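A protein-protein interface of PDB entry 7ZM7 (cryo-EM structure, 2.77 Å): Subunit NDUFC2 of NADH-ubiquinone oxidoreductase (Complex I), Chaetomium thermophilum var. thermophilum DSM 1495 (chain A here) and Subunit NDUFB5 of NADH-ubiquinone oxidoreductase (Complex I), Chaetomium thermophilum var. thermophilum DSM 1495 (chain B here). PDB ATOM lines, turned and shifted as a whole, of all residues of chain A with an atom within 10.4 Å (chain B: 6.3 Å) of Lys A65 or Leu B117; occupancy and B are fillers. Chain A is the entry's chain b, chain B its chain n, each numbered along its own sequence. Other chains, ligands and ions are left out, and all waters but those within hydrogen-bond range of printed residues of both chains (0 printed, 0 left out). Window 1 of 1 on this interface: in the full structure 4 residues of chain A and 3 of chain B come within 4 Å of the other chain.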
ATOM      1  N   GLN A  57      23.465 -18.270   4.643  1.00  0.00           N
ATOM      2  CA  GLN A  57      22.797 -17.004   4.915  1.00  0.00           C
ATOM      3  C   GLN A  57      23.780 -15.849   4.892  1.00  0.00           C
ATOM      4  O   GLN A  57      23.444 -14.742   4.460  1.00  0.00           O
ATOM      5  CB  GLN A  57      22.103 -17.075   6.267  1.00  0.00           C
ATOM      6  CG  GLN A  57      20.901 -17.979   6.292  1.00  0.00           C
ATOM      7  CD  GLN A  57      20.399 -18.232   7.680  1.00  0.00           C
ATOM      8  OE1 GLN A  57      19.292 -18.716   7.873  1.00  0.00           O
ATOM      9  NE2 GLN A  57      21.221 -17.917   8.664  1.00  0.00           N
ATOM     10  N   THR A  58      24.998 -16.087   5.378  1.00  0.00           N
ATOM     11  CA  THR A  58      26.030 -15.057   5.380  1.00  0.00           C
ATOM     12  C   THR A  58      26.411 -14.646   3.966  1.00  0.00           C
ATOM     13  O   THR A  58      26.642 -13.467   3.697  1.00  0.00           O
ATOM     14  CB  THR A  58      27.249 -15.567   6.137  1.00  0.00           C
ATOM     15  OG1 THR A  58      26.827 -16.102   7.393  1.00  0.00           O
ATOM     16  CG2 THR A  58      28.240 -14.446   6.371  1.00  0.00           C
ATOM     17  N   LYS A  59      26.513 -15.609   3.056  1.00  0.00           N
ATOM     18  CA  LYS A  59      26.804 -15.272   1.670  1.00  0.00           C
ATOM     19  C   LYS A  59      25.682 -14.445   1.067  1.00  0.00           C
ATOM     20  O   LYS A  59      25.930 -13.489   0.331  1.00  0.00           O
ATOM     21  CB  LYS A  59      27.032 -16.547   0.867  1.00  0.00           C
ATOM     22  CG  LYS A  59      28.464 -16.993   0.844  1.00  0.00           C
ATOM     23  CD  LYS A  59      28.704 -17.994  -0.267  1.00  0.00           C
ATOM     24  CE  LYS A  59      30.052 -17.769  -0.939  1.00  0.00           C
ATOM     25  NZ  LYS A  59      31.190 -18.040  -0.020  1.00  0.00           N
ATOM     26  N   MET A  60      24.440 -14.800   1.379  1.00  0.00           N
ATOM     27  CA  MET A  60      23.294 -14.111   0.810  1.00  0.00           C
ATOM     28  C   MET A  60      23.189 -12.686   1.335  1.00  0.00           C
ATOM     29  O   MET A  60      23.016 -11.740   0.563  1.00  0.00           O
ATOM     30  CB  MET A  60      22.035 -14.901   1.124  1.00  0.00           C
ATOM     31  CG  MET A  60      21.797 -15.987   0.148  1.00  0.00           C
ATOM     32  SD  MET A  60      20.725 -17.284   0.758  1.00  0.00           S
ATOM     33  CE  MET A  60      20.484 -18.194  -0.759  1.00  0.00           C
ATOM     34  N   LEU A  61      23.299 -12.510   2.645  1.00  0.00           N
ATOM     35  CA  LEU A  61      23.232 -11.164   3.186  1.00  0.00           C
ATOM     36  C   LEU A  61      24.401 -10.322   2.700  1.00  0.00           C
ATOM     37  O   LEU A  61      24.247  -9.120   2.465  1.00  0.00           O
ATOM     38  CB  LEU A  61      23.175 -11.216   4.708  1.00  0.00           C
ATOM     39  CG  LEU A  61      21.888 -11.872   5.208  1.00  0.00           C
ATOM     40  CD1 LEU A  61      21.919 -12.047   6.694  1.00  0.00           C
ATOM     41  CD2 LEU A  61      20.676 -11.080   4.792  1.00  0.00           C
ATOM     42  N   GLU A  62      25.571 -10.936   2.515  1.00  0.00           N
ATOM     43  CA  GLU A  62      26.695 -10.212   1.935  1.00  0.00           C
ATOM     44  C   GLU A  62      26.372  -9.718   0.534  1.00  0.00           C
ATOM     45  O   GLU A  62      26.509  -8.526   0.242  1.00  0.00           O
ATOM     46  CB  GLU A  62      27.938 -11.092   1.913  1.00  0.00           C
ATOM     47  CG  GLU A  62      28.729 -11.047   3.200  1.00  0.00           C
ATOM     48  CD  GLU A  62      29.199  -9.648   3.544  1.00  0.00           C
ATOM     49  OE1 GLU A  62      29.674  -8.937   2.633  1.00  0.00           O
ATOM     50  OE2 GLU A  62      29.085  -9.257   4.724  1.00  0.00           O
ATOM     51  N   GLU A  63      25.962 -10.624  -0.348  1.00  0.00           N
ATOM     52  CA  GLU A  63      25.555 -10.249  -1.728  1.00  0.00           C
ATOM     53  C   GLU A  63      24.528  -9.116  -1.695  1.00  0.00           C
ATOM     54  O   GLU A  63      24.713  -8.159  -2.447  1.00  0.00           O
ATOM     55  CB  GLU A  63      24.985 -11.460  -2.463  1.00  0.00           C
ATOM     56  CG  GLU A  63      26.017 -12.524  -2.780  1.00  0.00           C
ATOM     57  CD  GLU A  63      27.145 -12.081  -3.698  1.00  0.00           C
ATOM     58  OE1 GLU A  63      26.858 -11.425  -4.721  1.00  0.00           O
ATOM     59  OE2 GLU A  63      28.311 -12.389  -3.384  1.00  0.00           O
ATOM     60  N   ARG A  64      23.462  -9.241  -0.898  1.00  0.00           N
ATOM     61  CA  ARG A  64      22.375  -8.233  -0.887  1.00  0.00           C
ATOM     62  C   ARG A  64      22.931  -6.872  -0.467  1.00  0.00           C
ATOM     63  O   ARG A  64      22.562  -5.881  -1.088  1.00  0.00           O
ATOM     64  CB  ARG A  64      21.257  -8.678   0.056  1.00  0.00           C
ATOM     65  CG  ARG A  64      20.030  -7.783   0.047  1.00  0.00           C
ATOM     66  CD  ARG A  64      19.200  -7.980  -1.202  1.00  0.00           C
ATOM     67  NE  ARG A  64      18.034  -7.120  -1.150  1.00  0.00           N
ATOM     68  CZ  ARG A  64      17.862  -6.042  -1.896  1.00  0.00           C
ATOM     69  NH1 ARG A  64      18.771  -5.699  -2.790  1.00  0.00           N
ATOM     70  NH2 ARG A  64      16.768  -5.323  -1.755  1.00  0.00           N
ATOM     71  N   LYS A  65      23.802  -6.831   0.539  1.00  0.00           N
ATOM     72  CA  LYS A  65      24.286  -5.516   1.004  1.00  0.00           C
ATOM     73  C   LYS A  65      25.155  -4.909  -0.088  1.00  0.00           C
ATOM     74  O   LYS A  65      25.267  -3.695  -0.126  1.00  0.00           O
ATOM     75  CB  LYS A  65      25.036  -5.662   2.326  1.00  0.00           C
ATOM     76  CG  LYS A  65      24.152  -6.012   3.514  1.00  0.00           C
ATOM     77  CD  LYS A  65      24.911  -6.314   4.779  1.00  0.00           C
ATOM     78  CE  LYS A  65      25.940  -7.410   4.617  1.00  0.00           C
ATOM     79  NZ  LYS A  65      26.408  -7.918   5.926  1.00  0.00           N
ATOM     80  N   GLN A  66      25.727  -5.747  -0.952  1.00  0.00           N
ATOM     81  CA  GLN A  66      26.466  -5.210  -2.085  1.00  0.00           C
ATOM     82  C   GLN A  66      25.532  -4.761  -3.197  1.00  0.00           C
ATOM     83  O   GLN A  66      25.799  -3.763  -3.870  1.00  0.00           O
ATOM     84  CB  GLN A  66      27.453  -6.252  -2.582  1.00  0.00           C
ATOM     85  CG  GLN A  66      28.514  -6.558  -1.568  1.00  0.00           C
ATOM     86  CD  GLN A  66      29.356  -5.341  -1.251  1.00  0.00           C
ATOM     87  OE1 GLN A  66      29.267  -4.779  -0.160  1.00  0.00           O
ATOM     88  NE2 GLN A  66      30.169  -4.920  -2.208  1.00  0.00           N
ATOM     89  N   ALA A  67      24.420  -5.473  -3.391  1.00  0.00           N
ATOM     90  CA  ALA A  67      23.433  -5.057  -4.378  1.00  0.00           C
ATOM     91  C   ALA A  67      22.766  -3.740  -3.998  1.00  0.00           C
ATOM     92  O   ALA A  67      22.565  -2.874  -4.854  1.00  0.00           O
ATOM     93  CB  ALA A  67      22.385  -6.144  -4.563  1.00  0.00           C
ATOM     94  N   ILE A  68      22.393  -3.573  -2.731  1.00  0.00           N
ATOM     95  CA  ILE A  68      21.818  -2.298  -2.317  1.00  0.00           C
ATOM     96  C   ILE A  68      22.851  -1.196  -2.476  1.00  0.00           C
ATOM     97  O   ILE A  68      22.506  -0.020  -2.621  1.00  0.00           O
ATOM     98  CB  ILE A  68      21.275  -2.393  -0.872  1.00  0.00           C
ATOM     99  CG1 ILE A  68      20.454  -3.661  -0.675  1.00  0.00           C
ATOM    100  CG2 ILE A  68      20.382  -1.243  -0.545  1.00  0.00           C
ATOM    101  CD1 ILE A  68      20.279  -4.049   0.777  1.00  0.00           C
ATOM    102  N   LEU A  69      24.133  -1.554  -2.463  1.00  0.00           N
ATOM    103  CA  LEU A  69      25.183  -0.559  -2.643  1.00  0.00           C
ATOM    104  C   LEU A  69      25.491  -0.311  -4.113  1.00  0.00           C
ATOM    105  O   LEU A  69      26.266   0.589  -4.438  1.00  0.00           O
ATOM    106  CB  LEU A  69      26.439  -0.990  -1.896  1.00  0.00           C
ATOM    107  CG  LEU A  69      26.290  -0.798  -0.400  1.00  0.00           C
ATOM    108  CD1 LEU A  69      27.531  -1.208   0.328  1.00  0.00           C
ATOM    109  CD2 LEU A  69      25.941   0.623  -0.101  1.00  0.00           C
ATOM    110  N   GLU A  70      24.939  -1.120  -5.015  1.00  0.00           N
ATOM    111  CA  GLU A  70      24.958  -0.751  -6.427  1.00  0.00           C
ATOM    112  C   GLU A  70      23.753   0.101  -6.779  1.00  0.00           C
ATOM    113  O   GLU A  70      23.881   1.124  -7.454  1.00  0.00           O
ATOM    114  CB  GLU A  70      25.005  -1.989  -7.319  1.00  0.00           C
ATOM    115  CG  GLU A  70      25.882  -3.115  -6.823  1.00  0.00           C
ATOM    116  CD  GLU A  70      27.358  -2.750  -6.717  1.00  0.00           C
ATOM    117  OE1 GLU A  70      27.752  -1.639  -7.124  1.00  0.00           O
ATOM    118  OE2 GLU A  70      28.140  -3.587  -6.220  1.00  0.00           O
ATOM    119  N   LYS A  71      22.579  -0.295  -6.312  1.00  0.00           N
ATOM    120  CA  LYS A  71      21.374   0.448  -6.639  1.00  0.00           C
ATOM    121  C   LYS A  71      21.482   1.890  -6.167  1.00  0.00           C
ATOM    122  O   LYS A  71      21.164   2.821  -6.914  1.00  0.00           O
ATOM    123  CB  LYS A  71      20.164  -0.245  -6.021  1.00  0.00           C
ATOM    124  CG  LYS A  71      18.848   0.313  -6.480  1.00  0.00           C
ATOM    125  CD  LYS A  71      17.729  -0.678  -6.277  1.00  0.00           C
ATOM    126  CE  LYS A  71      16.396  -0.028  -6.572  1.00  0.00           C
ATOM    127  NZ  LYS A  71      16.424   0.648  -7.895  1.00  0.00           N
ATOM    128  N   ARG A  72      21.946   2.093  -4.937  1.00  0.00           N
ATOM    129  CA  ARG A  72      22.180   3.440  -4.446  1.00  0.00           C
ATOM    130  C   ARG A  72      23.289   4.126  -5.225  1.00  0.00           C
ATOM    131  O   ARG A  72      23.220   5.335  -5.469  1.00  0.00           O
ATOM    132  CB  ARG A  72      22.531   3.404  -2.968  1.00  0.00           C
ATOM    133  CG  ARG A  72      21.439   2.883  -2.072  1.00  0.00           C
ATOM    134  CD  ARG A  72      21.727   3.276  -0.657  1.00  0.00           C
ATOM    135  NE  ARG A  72      21.889   4.718  -0.541  1.00  0.00           N
ATOM    136  CZ  ARG A  72      20.880   5.580  -0.468  1.00  0.00           C
ATOM    137  NH1 ARG A  72      19.628   5.152  -0.499  1.00  0.00           N
ATOM    138  NH2 ARG A  72      21.123   6.874  -0.358  1.00  0.00           N
ATOM    139  N   ALA A  73      24.316   3.379  -5.625  1.00  0.00           N
ATOM    140  CA  ALA A  73      25.402   3.973  -6.388  1.00  0.00           C
ATOM    141  C   ALA A  73      24.968   4.316  -7.804  1.00  0.00           C
ATOM    142  O   ALA A  73      25.104   5.461  -8.239  1.00  0.00           O
ATOM    143  CB  ALA A  73      26.598   3.023  -6.415  1.00  0.00           C
ATOM    144  N   ALA B 112      25.871  -1.392  12.669  1.00  0.00           N
ATOM    145  CA  ALA B 112      24.963  -0.254  12.732  1.00  0.00           C
ATOM    146  C   ALA B 112      24.705   0.298  11.339  1.00  0.00           C
ATOM    147  O   ALA B 112      23.572   0.645  10.995  1.00  0.00           O
ATOM    148  CB  ALA B 112      25.536   0.827  13.638  1.00  0.00           C
ATOM    149  N   HIS B 113      25.749   0.342  10.508  1.00  0.00           N
ATOM    150  CA  HIS B 113      25.596   0.839   9.118  1.00  0.00           C
ATOM    151  C   HIS B 113      24.850  -0.200   8.285  1.00  0.00           C
ATOM    152  O   HIS B 113      23.988   0.208   7.477  1.00  0.00           O
ATOM    153  CB  HIS B 113      26.968   1.149   8.506  1.00  0.00           C
ATOM    154  CG  HIS B 113      27.016   0.963   7.028  1.00  0.00           C
ATOM    155  ND1 HIS B 113      26.453   1.867   6.151  1.00  0.00           N
ATOM    156  CD2 HIS B 113      27.547  -0.021   6.270  1.00  0.00           C
ATOM    157  CE1 HIS B 113      26.635   1.447   4.916  1.00  0.00           C
ATOM    158  NE2 HIS B 113      27.303   0.291   4.961  1.00  0.00           N
ATOM    159  N   ASP B 114      25.151  -1.487   8.477  1.00  0.00           N
ATOM    160  CA  ASP B 114      24.561  -2.517   7.635  1.00  0.00           C
ATOM    161  C   ASP B 114      23.083  -2.713   7.894  1.00  0.00           C
ATOM    162  O   ASP B 114      22.357  -3.100   6.978  1.00  0.00           O
ATOM    163  CB  ASP B 114      25.275  -3.844   7.839  1.00  0.00           C
ATOM    164  CG  ASP B 114      26.395  -4.047   6.867  1.00  0.00           C
ATOM    165  OD1 ASP B 114      26.610  -3.166   6.017  1.00  0.00           O
ATOM    166  OD2 ASP B 114      27.059  -5.098   6.947  1.00  0.00           O
ATOM    167  N   LYS B 115      22.633  -2.469   9.118  1.00  0.00           N
ATOM    168  CA  LYS B 115      21.224  -2.626   9.437  1.00  0.00           C
ATOM    169  C   LYS B 115      20.408  -1.467   8.888  1.00  0.00           C
ATOM    170  O   LYS B 115      19.271  -1.661   8.450  1.00  0.00           O
ATOM    171  CB  LYS B 115      21.060  -2.769  10.947  1.00  0.00           C
ATOM    172  CG  LYS B 115      19.749  -2.317  11.491  1.00  0.00           C
ATOM    173  CD  LYS B 115      19.835  -2.170  12.978  1.00  0.00           C
ATOM    174  CE  LYS B 115      18.644  -1.429  13.533  1.00  0.00           C
ATOM    175  NZ  LYS B 115      18.701  -1.376  15.017  1.00  0.00           N
ATOM    176  N   HIS B 116      20.970  -0.257   8.887  1.00  0.00           N
ATOM    177  CA  HIS B 116      20.343   0.841   8.158  1.00  0.00           C
ATOM    178  C   HIS B 116      20.216   0.528   6.675  1.00  0.00           C
ATOM    179  O   HIS B 116      19.193   0.826   6.060  1.00  0.00           O
ATOM    180  CB  HIS B 116      21.131   2.133   8.350  1.00  0.00           C
ATOM    181  CG  HIS B 116      20.894   2.814   9.657  1.00  0.00           C
ATOM    182  ND1 HIS B 116      21.652   3.878  10.083  1.00  0.00           N
ATOM    183  CD2 HIS B 116      19.946   2.629  10.598  1.00  0.00           C
ATOM    184  CE1 HIS B 116      21.197   4.302  11.246  1.00  0.00           C
ATOM    185  NE2 HIS B 116      20.161   3.561  11.580  1.00  0.00           N
ATOM    186  N   LEU B 117      21.258   0.003   6.051  1.00  0.00           N
ATOM    187  CA  LEU B 117      21.244  -0.279   4.591  1.00  0.00           C
ATOM    188  C   LEU B 117      20.160  -1.306   4.265  1.00  0.00           C
ATOM    189  O   LEU B 117      19.395  -1.077   3.333  1.00  0.00           O
ATOM    190  CB  LEU B 117      22.626  -0.807   4.211  1.00  0.00           C
ATOM    191  CG  LEU B 117      22.837  -1.159   2.744  1.00  0.00           C
ATOM    192  CD1 LEU B 117      22.943   0.100   1.899  1.00  0.00           C
ATOM    193  CD2 LEU B 117      24.083  -2.009   2.589  1.00  0.00           C
ATOM    194  N   LEU B 118      20.051  -2.371   4.998  1.00  0.00           N
ATOM    195  CA  LEU B 118      19.076  -3.440   4.688  1.00  0.00           C
ATOM    196  C   LEU B 118      17.655  -3.008   5.055  1.00  0.00           C
ATOM    197  O   LEU B 118      16.734  -3.389   4.330  1.00  0.00           O
ATOM    198  CB  LEU B 118      19.486  -4.719   5.414  1.00  0.00           C
ATOM    199  CG  LEU B 118      20.700  -5.458   4.862  1.00  0.00           C
ATOM    200  CD1 LEU B 118      21.344  -6.304   5.948  1.00  0.00           C
ATOM    201  CD2 LEU B 118      20.313  -6.325   3.678  1.00  0.00           C
ATOM    202  N   LEU B 119      17.507  -2.211   6.130  1.00  0.00           N
ATOM    203  CA  LEU B 119      16.137  -1.845   6.580  1.00  0.00           C
ATOM    204  C   LEU B 119      15.603  -0.593   5.881  1.00  0.00           C
ATOM    205  O   LEU B 119      14.476  -0.197   6.208  1.00  0.00           O
ATOM    206  CB  LEU B 119      16.166  -1.647   8.101  1.00  0.00           C
ATOM    207  CG  LEU B 119      15.143  -2.415   8.925  1.00  0.00           C
ATOM    208  CD1 LEU B 119      15.116  -3.878   8.530  1.00  0.00           C
ATOM    209  CD2 LEU B 119      15.468  -2.275  10.399  1.00  0.00           C
ATOM    210  N   THR B 120      16.407   0.047   5.036  1.00  0.00           N
ATOM    211  CA  THR B 120      15.994   1.340   4.428  1.00  0.00           C
ATOM    212  C   THR B 120      16.115   1.175   2.923  1.00  0.00           C
ATOM    213  O   THR B 120      16.420   2.172   2.255  1.00  0.00           O
ATOM    214  CB  THR B 120      16.736   2.569   4.971  1.00  0.00           C
ATOM    215  OG1 THR B 120      18.103   2.525   4.566  1.00  0.00           O
ATOM    216  CG2 THR B 120      16.612   2.751   6.468  1.00  0.00           C
ATOM    217  N   ALA B 121      15.848  -0.020   2.418  1.00  0.00           N
ATOM    218  CA  ALA B 121      16.075  -0.291   0.989  1.00  0.00           C
ATOM    219  C   ALA B 121      14.870   0.159   0.170  1.00  0.00           C
ATOM    220  O   ALA B 121      13.791   0.300   0.739  1.00  0.00           O
ATOM    221  CB  ALA B 121      16.429  -1.741   0.798  1.00  0.00           C
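Lys A65 touches just these residues of chain B: Asp B114, Leu B117 and Leu B118. Of chain A, only Lys A65, Ile A68 and Leu A69 come within 4 Å of Leu B117. No residue of chain A comes within 4 Å of His B113. Asp B114 touches just one residue of chain A: Lys A65. Leu B118 touches just these residues of chain A: Arg A64 (3.9 Å), Lys A65 (3.7 Å) and Ile A68 (3.7 Å). No residue of chain A comes within 4 Å of Thr B120. Of the printed residues of chain B, Leu A69 touches Leu B117. Of the printed residues of chain B, Arg A64 touches Leu B118. Lys B115 touches none of the printed residues of chain A. The nearest residue of chain B that does not touch Lys A65 is Lys B115 (6.2 Å). The nearest residue of chain A that does not touch Leu B117 is Arg A72 (4.3 Å).
The side-chain amino group of Lys A65 is in salt-bridge range of the side-chain carboxylate of Asp B114 (3.1 Å).
The side-chain amino group (NZ) of Lys A65 is in salt-bridge range of the side-chain carboxylate (OE2) of Glu A62 (3.2 Å).
Arg A64 touches Leu B118. Lys A65 touches Leu B117. CG of Lys A65 touches CD1 of Leu B118 (3.7 Å). Ile A68 touches Leu B117 (CG2 to CD1, 3.8 Å). CD1 of Ile A68 touches CD2 of Leu B118 (3.7 Å). Leu B117 touches Leu A69 (CD1 to CD2, 3.6 Å).
Of the 10 printed residues of chain B, 3 touch a printed residue of chain A. Hydrophobic or aromatic side chains of chain A that line the printed part of chain B: Ile A68 and Leu A69. Among the printed residues, Asp or Glu carboxylates within 4 Å of a Lys or Arg side-chain nitrogen of the other chain: Lys A65 with Asp B114 (3.1 Å).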
